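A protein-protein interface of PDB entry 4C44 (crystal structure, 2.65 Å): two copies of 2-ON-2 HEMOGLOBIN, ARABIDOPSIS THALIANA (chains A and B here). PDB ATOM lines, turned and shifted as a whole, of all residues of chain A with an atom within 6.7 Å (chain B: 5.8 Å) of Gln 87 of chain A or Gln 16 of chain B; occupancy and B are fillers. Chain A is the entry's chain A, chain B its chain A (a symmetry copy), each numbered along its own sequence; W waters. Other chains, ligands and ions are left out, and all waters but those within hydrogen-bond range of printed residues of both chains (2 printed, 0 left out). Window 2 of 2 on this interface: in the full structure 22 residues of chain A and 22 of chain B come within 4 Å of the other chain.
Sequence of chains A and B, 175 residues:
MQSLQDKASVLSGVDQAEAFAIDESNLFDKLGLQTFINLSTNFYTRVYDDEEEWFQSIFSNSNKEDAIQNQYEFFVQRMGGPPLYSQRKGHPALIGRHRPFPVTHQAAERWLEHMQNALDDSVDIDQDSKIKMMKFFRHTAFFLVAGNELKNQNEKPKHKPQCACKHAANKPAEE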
ATOM      1  N   GLN A  77      -3.358   1.190 -23.075  1.00  0.00           N
ATOM      2  CA  GLN A  77      -4.226   0.992 -24.234  1.00  0.00           C
ATOM      3  C   GLN A  77      -5.021   2.251 -24.507  1.00  0.00           C
ATOM      4  O   GLN A  77      -5.135   2.660 -25.649  1.00  0.00           O
ATOM      5  CB  GLN A  77      -5.199  -0.165 -24.022  1.00  0.00           C
ATOM      6  CG  GLN A  77      -6.150  -0.416 -25.191  1.00  0.00           C
ATOM      7  CD  GLN A  77      -6.915  -1.728 -25.063  1.00  0.00           C
ATOM      8  OE1 GLN A  77      -8.146  -1.750 -25.069  1.00  0.00           O
ATOM      9  NE2 GLN A  77      -6.182  -2.831 -24.948  1.00  0.00           N
ATOM     10  N   PRO A  83      -2.659  -1.874 -27.779  1.00  0.00           N
ATOM     11  CA  PRO A  83      -3.804  -2.426 -27.053  1.00  0.00           C
ATOM     12  C   PRO A  83      -3.451  -3.682 -26.243  1.00  0.00           C
ATOM     13  O   PRO A  83      -3.877  -4.795 -26.573  1.00  0.00           O
ATOM     14  CB  PRO A  83      -4.808  -2.735 -28.167  1.00  0.00           C
ATOM     15  CG  PRO A  83      -3.965  -2.982 -29.362  1.00  0.00           C
ATOM     16  CD  PRO A  83      -2.781  -2.072 -29.233  1.00  0.00           C
ATOM     17  N   LEU A  84      -2.679  -3.499 -25.177  1.00  0.00           N
ATOM     18  CA  LEU A  84      -2.281  -4.636 -24.344  1.00  0.00           C
ATOM     19  C   LEU A  84      -3.463  -5.270 -23.608  1.00  0.00           C
ATOM     20  O   LEU A  84      -3.601  -6.492 -23.578  1.00  0.00           O
ATOM     21  CB  LEU A  84      -1.176  -4.236 -23.373  1.00  0.00           C
ATOM     22  CG  LEU A  84       0.172  -3.781 -23.970  1.00  0.00           C
ATOM     23  CD1 LEU A  84       1.175  -3.482 -22.858  1.00  0.00           C
ATOM     24  CD2 LEU A  84       0.730  -4.815 -24.939  1.00  0.00           C
ATOM     25  N   TYR A  85      -4.321  -4.440 -23.026  1.00  0.00           N
ATOM     26  CA  TYR A  85      -5.465  -4.947 -22.259  1.00  0.00           C
ATOM     27  C   TYR A  85      -6.370  -5.873 -23.094  1.00  0.00           C
ATOM     28  O   TYR A  85      -6.647  -7.007 -22.688  1.00  0.00           O
ATOM     29  CB  TYR A  85      -6.285  -3.802 -21.659  1.00  0.00           C
ATOM     30  CG  TYR A  85      -7.346  -4.299 -20.705  1.00  0.00           C
ATOM     31  CD1 TYR A  85      -8.605  -4.682 -21.172  1.00  0.00           C
ATOM     32  CD2 TYR A  85      -7.083  -4.414 -19.339  1.00  0.00           C
ATOM     33  CE1 TYR A  85      -9.562  -5.164 -20.312  1.00  0.00           C
ATOM     34  CE2 TYR A  85      -8.049  -4.889 -18.466  1.00  0.00           C
ATOM     35  CZ  TYR A  85      -9.281  -5.266 -18.962  1.00  0.00           C
ATOM     36  OH  TYR A  85     -10.241  -5.756 -18.107  1.00  0.00           O
ATOM     37  N   SER A  86      -6.834  -5.382 -24.238  1.00  0.00           N
ATOM     38  CA  SER A  86      -7.722  -6.146 -25.095  1.00  0.00           C
ATOM     39  C   SER A  86      -7.071  -7.436 -25.570  1.00  0.00           C
ATOM     40  O   SER A  86      -7.700  -8.494 -25.488  1.00  0.00           O
ATOM     41  CB  SER A  86      -8.198  -5.311 -26.283  1.00  0.00           C
ATOM     42  OG  SER A  86      -9.281  -4.484 -25.896  1.00  0.00           O
ATOM     43  N   GLN A  87      -5.816  -7.345 -26.035  1.00  0.00           N
ATOM     44  CA  GLN A  87      -5.002  -8.521 -26.436  1.00  0.00           C
ATOM     45  C   GLN A  87      -5.173  -9.671 -25.455  1.00  0.00           C
ATOM     46  O   GLN A  87      -5.230 -10.829 -25.853  1.00  0.00           O
ATOM     47  CB  GLN A  87      -3.512  -8.166 -26.580  1.00  0.00           C
ATOM     48  CG  GLN A  87      -2.658  -9.270 -27.229  1.00  0.00           C
ATOM     49  CD  GLN A  87      -1.148  -8.967 -27.276  1.00  0.00           C
ATOM     50  OE1 GLN A  87      -0.533  -8.578 -26.269  1.00  0.00           O
ATOM     51  NE2 GLN A  87      -0.545  -9.164 -28.445  1.00  0.00           N
ATOM     52  N   ARG A  88      -5.317  -9.318 -24.184  1.00  0.00           N
ATOM     53  CA  ARG A  88      -5.319 -10.251 -23.073  1.00  0.00           C
ATOM     54  C   ARG A  88      -6.703 -10.524 -22.520  1.00  0.00           C
ATOM     55  O   ARG A  88      -7.011 -11.650 -22.165  1.00  0.00           O
ATOM     56  CB  ARG A  88      -4.498  -9.634 -21.959  1.00  0.00           C
ATOM     57  CG  ARG A  88      -3.829 -10.577 -21.006  1.00  0.00           C
ATOM     58  CD  ARG A  88      -2.914  -9.755 -20.105  1.00  0.00           C
ATOM     59  NE  ARG A  88      -3.463  -9.769 -18.763  1.00  0.00           N
ATOM     60  CZ  ARG A  88      -3.780  -8.711 -18.032  1.00  0.00           C
ATOM     61  NH1 ARG A  88      -3.580  -7.482 -18.473  1.00  0.00           N
ATOM     62  NH2 ARG A  88      -4.283  -8.904 -16.828  1.00  0.00           N
ATOM     63  N   LYS A  89      -7.537  -9.495 -22.393  1.00  0.00           N
ATOM     64  CA  LYS A  89      -8.810  -9.675 -21.675  1.00  0.00           C
ATOM     65  C   LYS A  89     -10.050  -9.317 -22.493  1.00  0.00           C
ATOM     66  O   LYS A  89     -11.178  -9.567 -22.042  1.00  0.00           O
ATOM     67  CB  LYS A  89      -8.813  -8.912 -20.335  1.00  0.00           C
ATOM     68  CG  LYS A  89      -7.640  -9.222 -19.432  1.00  0.00           C
ATOM     69  CD  LYS A  89      -7.843  -8.702 -18.027  1.00  0.00           C
ATOM     70  CE  LYS A  89      -8.750  -9.618 -17.238  1.00  0.00           C
ATOM     71  NZ  LYS A  89      -8.769  -9.235 -15.802  1.00  0.00           N
ATOM     72  N   GLY A  90      -9.849  -8.736 -23.674  1.00  0.00           N
ATOM     73  CA  GLY A  90     -10.969  -8.256 -24.451  1.00  0.00           C
ATOM     74  C   GLY A  90     -11.389  -6.821 -24.136  1.00  0.00           C
ATOM     75  O   GLY A  90     -10.536  -5.933 -23.951  1.00  0.00           O
ATOM     76  N   HIS A  91     -12.702  -6.589 -24.105  1.00  0.00           N
ATOM     77  CA  HIS A  91     -13.257  -5.245 -23.920  1.00  0.00           C
ATOM     78  C   HIS A  91     -12.984  -4.777 -22.510  1.00  0.00           C
ATOM     79  O   HIS A  91     -13.104  -5.567 -21.573  1.00  0.00           O
ATOM     80  CB  HIS A  91     -14.759  -5.235 -24.163  1.00  0.00           C
ATOM     81  CG  HIS A  91     -15.112  -5.418 -25.590  1.00  0.00           C
ATOM     82  ND1 HIS A  91     -14.700  -4.539 -26.571  1.00  0.00           N
ATOM     83  CD2 HIS A  91     -15.796  -6.397 -26.224  1.00  0.00           C
ATOM     84  CE1 HIS A  91     -15.123  -4.964 -27.748  1.00  0.00           C
ATOM     85  NE2 HIS A  91     -15.790  -6.092 -27.568  1.00  0.00           N
ATOM     86  N   GLN B   5     -14.944 -12.788 -20.642  1.00  0.00           N
ATOM     87  CA  GLN B   5     -14.331 -13.154 -21.910  1.00  0.00           C
ATOM     88  C   GLN B   5     -14.238 -14.677 -22.104  1.00  0.00           C
ATOM     89  O   GLN B   5     -14.223 -15.141 -23.245  1.00  0.00           O
ATOM     90  CB  GLN B   5     -12.968 -12.456 -22.117  1.00  0.00           C
ATOM     91  CG  GLN B   5     -11.878 -12.776 -21.098  1.00  0.00           C
ATOM     92  CD  GLN B   5     -12.036 -12.009 -19.787  1.00  0.00           C
ATOM     93  OE1 GLN B   5     -13.124 -11.549 -19.452  1.00  0.00           O
ATOM     94  NE2 GLN B   5     -10.952 -11.893 -19.029  1.00  0.00           N
ATOM     95  N   SER B   9     -16.118 -16.893 -25.190  1.00  0.00           N
ATOM     96  CA  SER B   9     -15.414 -17.824 -26.047  1.00  0.00           C
ATOM     97  C   SER B   9     -16.129 -19.156 -26.102  1.00  0.00           C
ATOM     98  O   SER B   9     -16.309 -19.733 -27.173  1.00  0.00           O
ATOM     99  CB  SER B   9     -13.991 -18.003 -25.551  1.00  0.00           C
ATOM    100  OG  SER B   9     -13.264 -16.809 -25.772  1.00  0.00           O
ATOM    101  N   VAL B  14     -15.584 -18.499 -30.586  1.00  0.00           N
ATOM    102  CA  VAL B  14     -14.513 -17.608 -31.028  1.00  0.00           C
ATOM    103  C   VAL B  14     -13.560 -17.349 -29.866  1.00  0.00           C
ATOM    104  O   VAL B  14     -13.955 -16.820 -28.810  1.00  0.00           O
ATOM    105  CB  VAL B  14     -15.063 -16.265 -31.569  1.00  0.00           C
ATOM    106  CG1 VAL B  14     -13.932 -15.379 -32.078  1.00  0.00           C
ATOM    107  CG2 VAL B  14     -16.071 -16.506 -32.677  1.00  0.00           C
ATOM    108  N   ASP B  15     -12.309 -17.742 -30.073  1.00  0.00           N
ATOM    109  CA  ASP B  15     -11.225 -17.538 -29.113  1.00  0.00           C
ATOM    110  C   ASP B  15     -10.994 -16.034 -28.913  1.00  0.00           C
ATOM    111  O   ASP B  15     -11.001 -15.285 -29.902  1.00  0.00           O
ATOM    112  CB  ASP B  15      -9.980 -18.184 -29.719  1.00  0.00           C
ATOM    113  CG  ASP B  15      -8.943 -18.531 -28.696  1.00  0.00           C
ATOM    114  OD1 ASP B  15      -8.422 -17.598 -28.035  1.00  0.00           O
ATOM    115  OD2 ASP B  15      -8.634 -19.742 -28.588  1.00  0.00           O
ATOM    116  N   GLN B  16     -10.792 -15.568 -27.676  1.00  0.00           N
ATOM    117  CA  GLN B  16     -10.607 -14.113 -27.468  1.00  0.00           C
ATOM    118  C   GLN B  16      -9.445 -13.543 -28.285  1.00  0.00           C
ATOM    119  O   GLN B  16      -9.513 -12.412 -28.771  1.00  0.00           O
ATOM    120  CB  GLN B  16     -10.510 -13.714 -25.982  1.00  0.00           C
ATOM    121  CG  GLN B  16      -9.131 -13.777 -25.347  1.00  0.00           C
ATOM    122  CD  GLN B  16      -8.238 -12.614 -25.733  1.00  0.00           C
ATOM    123  OE1 GLN B  16      -8.670 -11.469 -25.767  1.00  0.00           O
ATOM    124  NE2 GLN B  16      -6.979 -12.911 -26.039  1.00  0.00           N
ATOM    125  N   ALA B  17      -8.392 -14.339 -28.439  1.00  0.00           N
ATOM    126  CA  ALA B  17      -7.279 -14.008 -29.318  1.00  0.00           C
ATOM    127  C   ALA B  17      -7.763 -13.671 -30.720  1.00  0.00           C
ATOM    128  O   ALA B  17      -7.400 -12.626 -31.256  1.00  0.00           O
ATOM    129  CB  ALA B  17      -6.279 -15.159 -29.371  1.00  0.00           C
ATOM    130  N   GLU B  18      -8.563 -14.566 -31.310  1.00  0.00           N
ATOM    131  CA  GLU B  18      -9.164 -14.349 -32.628  1.00  0.00           C
ATOM    132  C   GLU B  18      -9.985 -13.074 -32.618  1.00  0.00           C
ATOM    133  O   GLU B  18      -9.879 -12.251 -33.523  1.00  0.00           O
ATOM    134  CB  GLU B  18     -10.113 -15.481 -32.989  1.00  0.00           C
ATOM    135  CG  GLU B  18      -9.514 -16.742 -33.562  1.00  0.00           C
ATOM    136  CD  GLU B  18     -10.612 -17.717 -33.963  1.00  0.00           C
ATOM    137  OE1 GLU B  18     -11.264 -18.325 -33.072  1.00  0.00           O
ATOM    138  OE2 GLU B  18     -10.843 -17.856 -35.186  1.00  0.00           O
ATOM    139  N   ALA B  19     -10.803 -12.922 -31.582  1.00  0.00           N
ATOM    140  CA  ALA B  19     -11.724 -11.794 -31.477  1.00  0.00           C
ATOM    141  C   ALA B  19     -11.034 -10.456 -31.623  1.00  0.00           C
ATOM    142  O   ALA B  19     -11.575  -9.575 -32.261  1.00  0.00           O
ATOM    143  CB  ALA B  19     -12.486 -11.849 -30.166  1.00  0.00           C
ATOM    144  N   PHE B  20      -9.838 -10.321 -31.046  1.00  0.00           N
ATOM    145  CA  PHE B  20      -9.094  -9.052 -31.080  1.00  0.00           C
ATOM    146  C   PHE B  20      -7.949  -8.970 -32.096  1.00  0.00           C
ATOM    147  O   PHE B  20      -7.103  -8.079 -32.032  1.00  0.00           O
ATOM    148  CB  PHE B  20      -8.726  -8.606 -29.656  1.00  0.00           C
ATOM    149  CG  PHE B  20      -9.933  -8.225 -28.865  1.00  0.00           C
ATOM    150  CD1 PHE B  20     -10.662  -9.195 -28.165  1.00  0.00           C
ATOM    151  CD2 PHE B  20     -10.433  -6.923 -28.916  1.00  0.00           C
ATOM    152  CE1 PHE B  20     -11.828  -8.854 -27.480  1.00  0.00           C
ATOM    153  CE2 PHE B  20     -11.605  -6.581 -28.233  1.00  0.00           C
ATOM    154  CZ  PHE B  20     -12.297  -7.547 -27.513  1.00  0.00           C
ATOM    155  N   ALA B  21      -7.977  -9.868 -33.074  1.00  0.00           N
ATOM    156  CA  ALA B  21      -7.040  -9.826 -34.193  1.00  0.00           C
ATOM    157  C   ALA B  21      -7.220  -8.545 -35.002  1.00  0.00           C
ATOM    158  O   ALA B  21      -6.292  -8.112 -35.688  1.00  0.00           O
ATOM    159  CB  ALA B  21      -7.176 -11.064 -35.074  1.00  0.00           C
ATOM    160  N   ASP B  23      -6.808  -5.812 -33.967  1.00  0.00           N
ATOM    161  CA  ASP B  23      -5.762  -4.898 -33.491  1.00  0.00           C
ATOM    162  C   ASP B  23      -4.381  -5.070 -34.149  1.00  0.00           C
ATOM    163  O   ASP B  23      -3.431  -4.389 -33.767  1.00  0.00           O
ATOM    164  CB  ASP B  23      -5.615  -4.997 -31.963  1.00  0.00           C
ATOM    165  CG  ASP B  23      -6.767  -4.341 -31.214  1.00  0.00           C
ATOM    166  OD1 ASP B  23      -7.363  -3.366 -31.743  1.00  0.00           O
ATOM    167  OD2 ASP B  23      -7.087  -4.798 -30.096  1.00  0.00           O
ATOM    168  N   HIS B 139     -17.641 -12.781 -31.009  1.00  0.00           N
ATOM    169  CA  HIS B 139     -17.134 -12.877 -29.663  1.00  0.00           C
ATOM    170  C   HIS B 139     -17.814 -11.848 -28.775  1.00  0.00           C
ATOM    171  O   HIS B 139     -18.205 -12.155 -27.642  1.00  0.00           O
ATOM    172  CB  HIS B 139     -15.620 -12.667 -29.626  1.00  0.00           C
ATOM    173  CG  HIS B 139     -15.053 -12.685 -28.235  1.00  0.00           C
ATOM    174  ND1 HIS B 139     -14.578 -13.838 -27.639  1.00  0.00           N
ATOM    175  CD2 HIS B 139     -14.916 -11.697 -27.312  1.00  0.00           C
ATOM    176  CE1 HIS B 139     -14.162 -13.554 -26.415  1.00  0.00           C
ATOM    177  NE2 HIS B 139     -14.360 -12.266 -26.192  1.00  0.00           N
HETATM  178  O   HOH W   1     -11.262 -11.253 -15.922  1.00  0.00           O
HETATM  179  O   HOH W   2      -5.426  -6.131 -28.630  1.00  0.00           O
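The side-chain amide oxygen (OE1) of Gln 16 of chain B lies close to the backbone carbonyl oxygen (O) of Ser 86 of chain A, 3.1 Å away. NE2 of Gln 16 of chain B lies within hydrogen-bond range of O of Gln 87 of chain A.
O of Pro 83 of chain A sits close to NE2 of Gln 77 of chain A, at 3.4 Å. NE2 of Gln 77 of chain A lies close to N of Ser 86 of chain A (2.7 Å). O of Gly 90 of chain A sits at hydrogen-bond distance from OG of Ser 86 of chain A, 2.7 Å away. O of Gln 5 of chain B sits at hydrogen-bond distance from OG of Ser 9 of chain B. The backbone NH (N) of Gln 16 of chain B sits at hydrogen-bond distance from the side-chain hydroxyl (OG) of Ser 9 of chain B, at 3.4 Å.
CG of Asp 23 of chain B touches CG of Pro 83 of chain A (3.6 Å). CB of Ser 86 of chain A touches CD2 of Phe 20 of chain B (3.8 Å). CD of Gln 16 of chain B touches O of Arg 88 of chain A, at 3.9 Å. Lys 89 of chain A touches Gln 5 of chain B. Gly 90 of chain A touches Gln 16 of chain B (N to OE1, 3.6 Å). Phe 20 of chain B touches Gly 90 of chain A. His 91 of chain A touches Phe 20 of chain B.
Printed residues of chain B within 4 Å of Gln 87 of chain A: Gln 16. Printed residues of chain A within 4 Å of Gln 16 of chain B: Ser 86, Gln 87, Arg 88 and Gly 90. Printed residues of chain B within 4 Å of Ser 86 of chain A: Gln 16 and Phe 20. Of the printed residues of chain B, Arg 88 of chain A touches Gln 16 (3.9 Å). Leu 84 of chain A touches none of the printed residues of chain B. Gln 77 of chain A touches none of the printed residues of chain B. The nearest residue of chain B that does not touch Gln 87 of chain A is Phe 20 of chain B (4.8 Å). The nearest residue of chain A that does not touch Gln 16 of chain B is Lys 89 of chain A (4.1 Å).
Of the 10 printed residues of chain A, 7 touch a printed residue of chain B. Printed residues of chain A that touch a printed residue of chain B: Pro 83, Ser 86, Gln 87, Arg 88, Lys 89, Gly 90 and His 91. Hydrophobic or aromatic side chains of chain A within 4 Å of the printed part of chain B: Pro 83 and His 91. Hydrophobic or aromatic side chains of chain B within 4 Å of the printed part of chain A: Phe 20. Among the printed residues, 9 pairs touch across the chains.
No position is printed for both chains.
Water W2 lies within hydrogen-bond range of OD2 of Asp 23 of chain B (2.6 Å), N of Gln 87 of chain A (2.9 Å) and O of Pro 83 of chain A (2.9 Å). Water W1 bridges the side-chain amide nitrogen (NE2) of Gln 5 of chain B (3.2 Å) and the side-chain amino group (NZ) of Lys 89 of chain A (3.2 Å).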
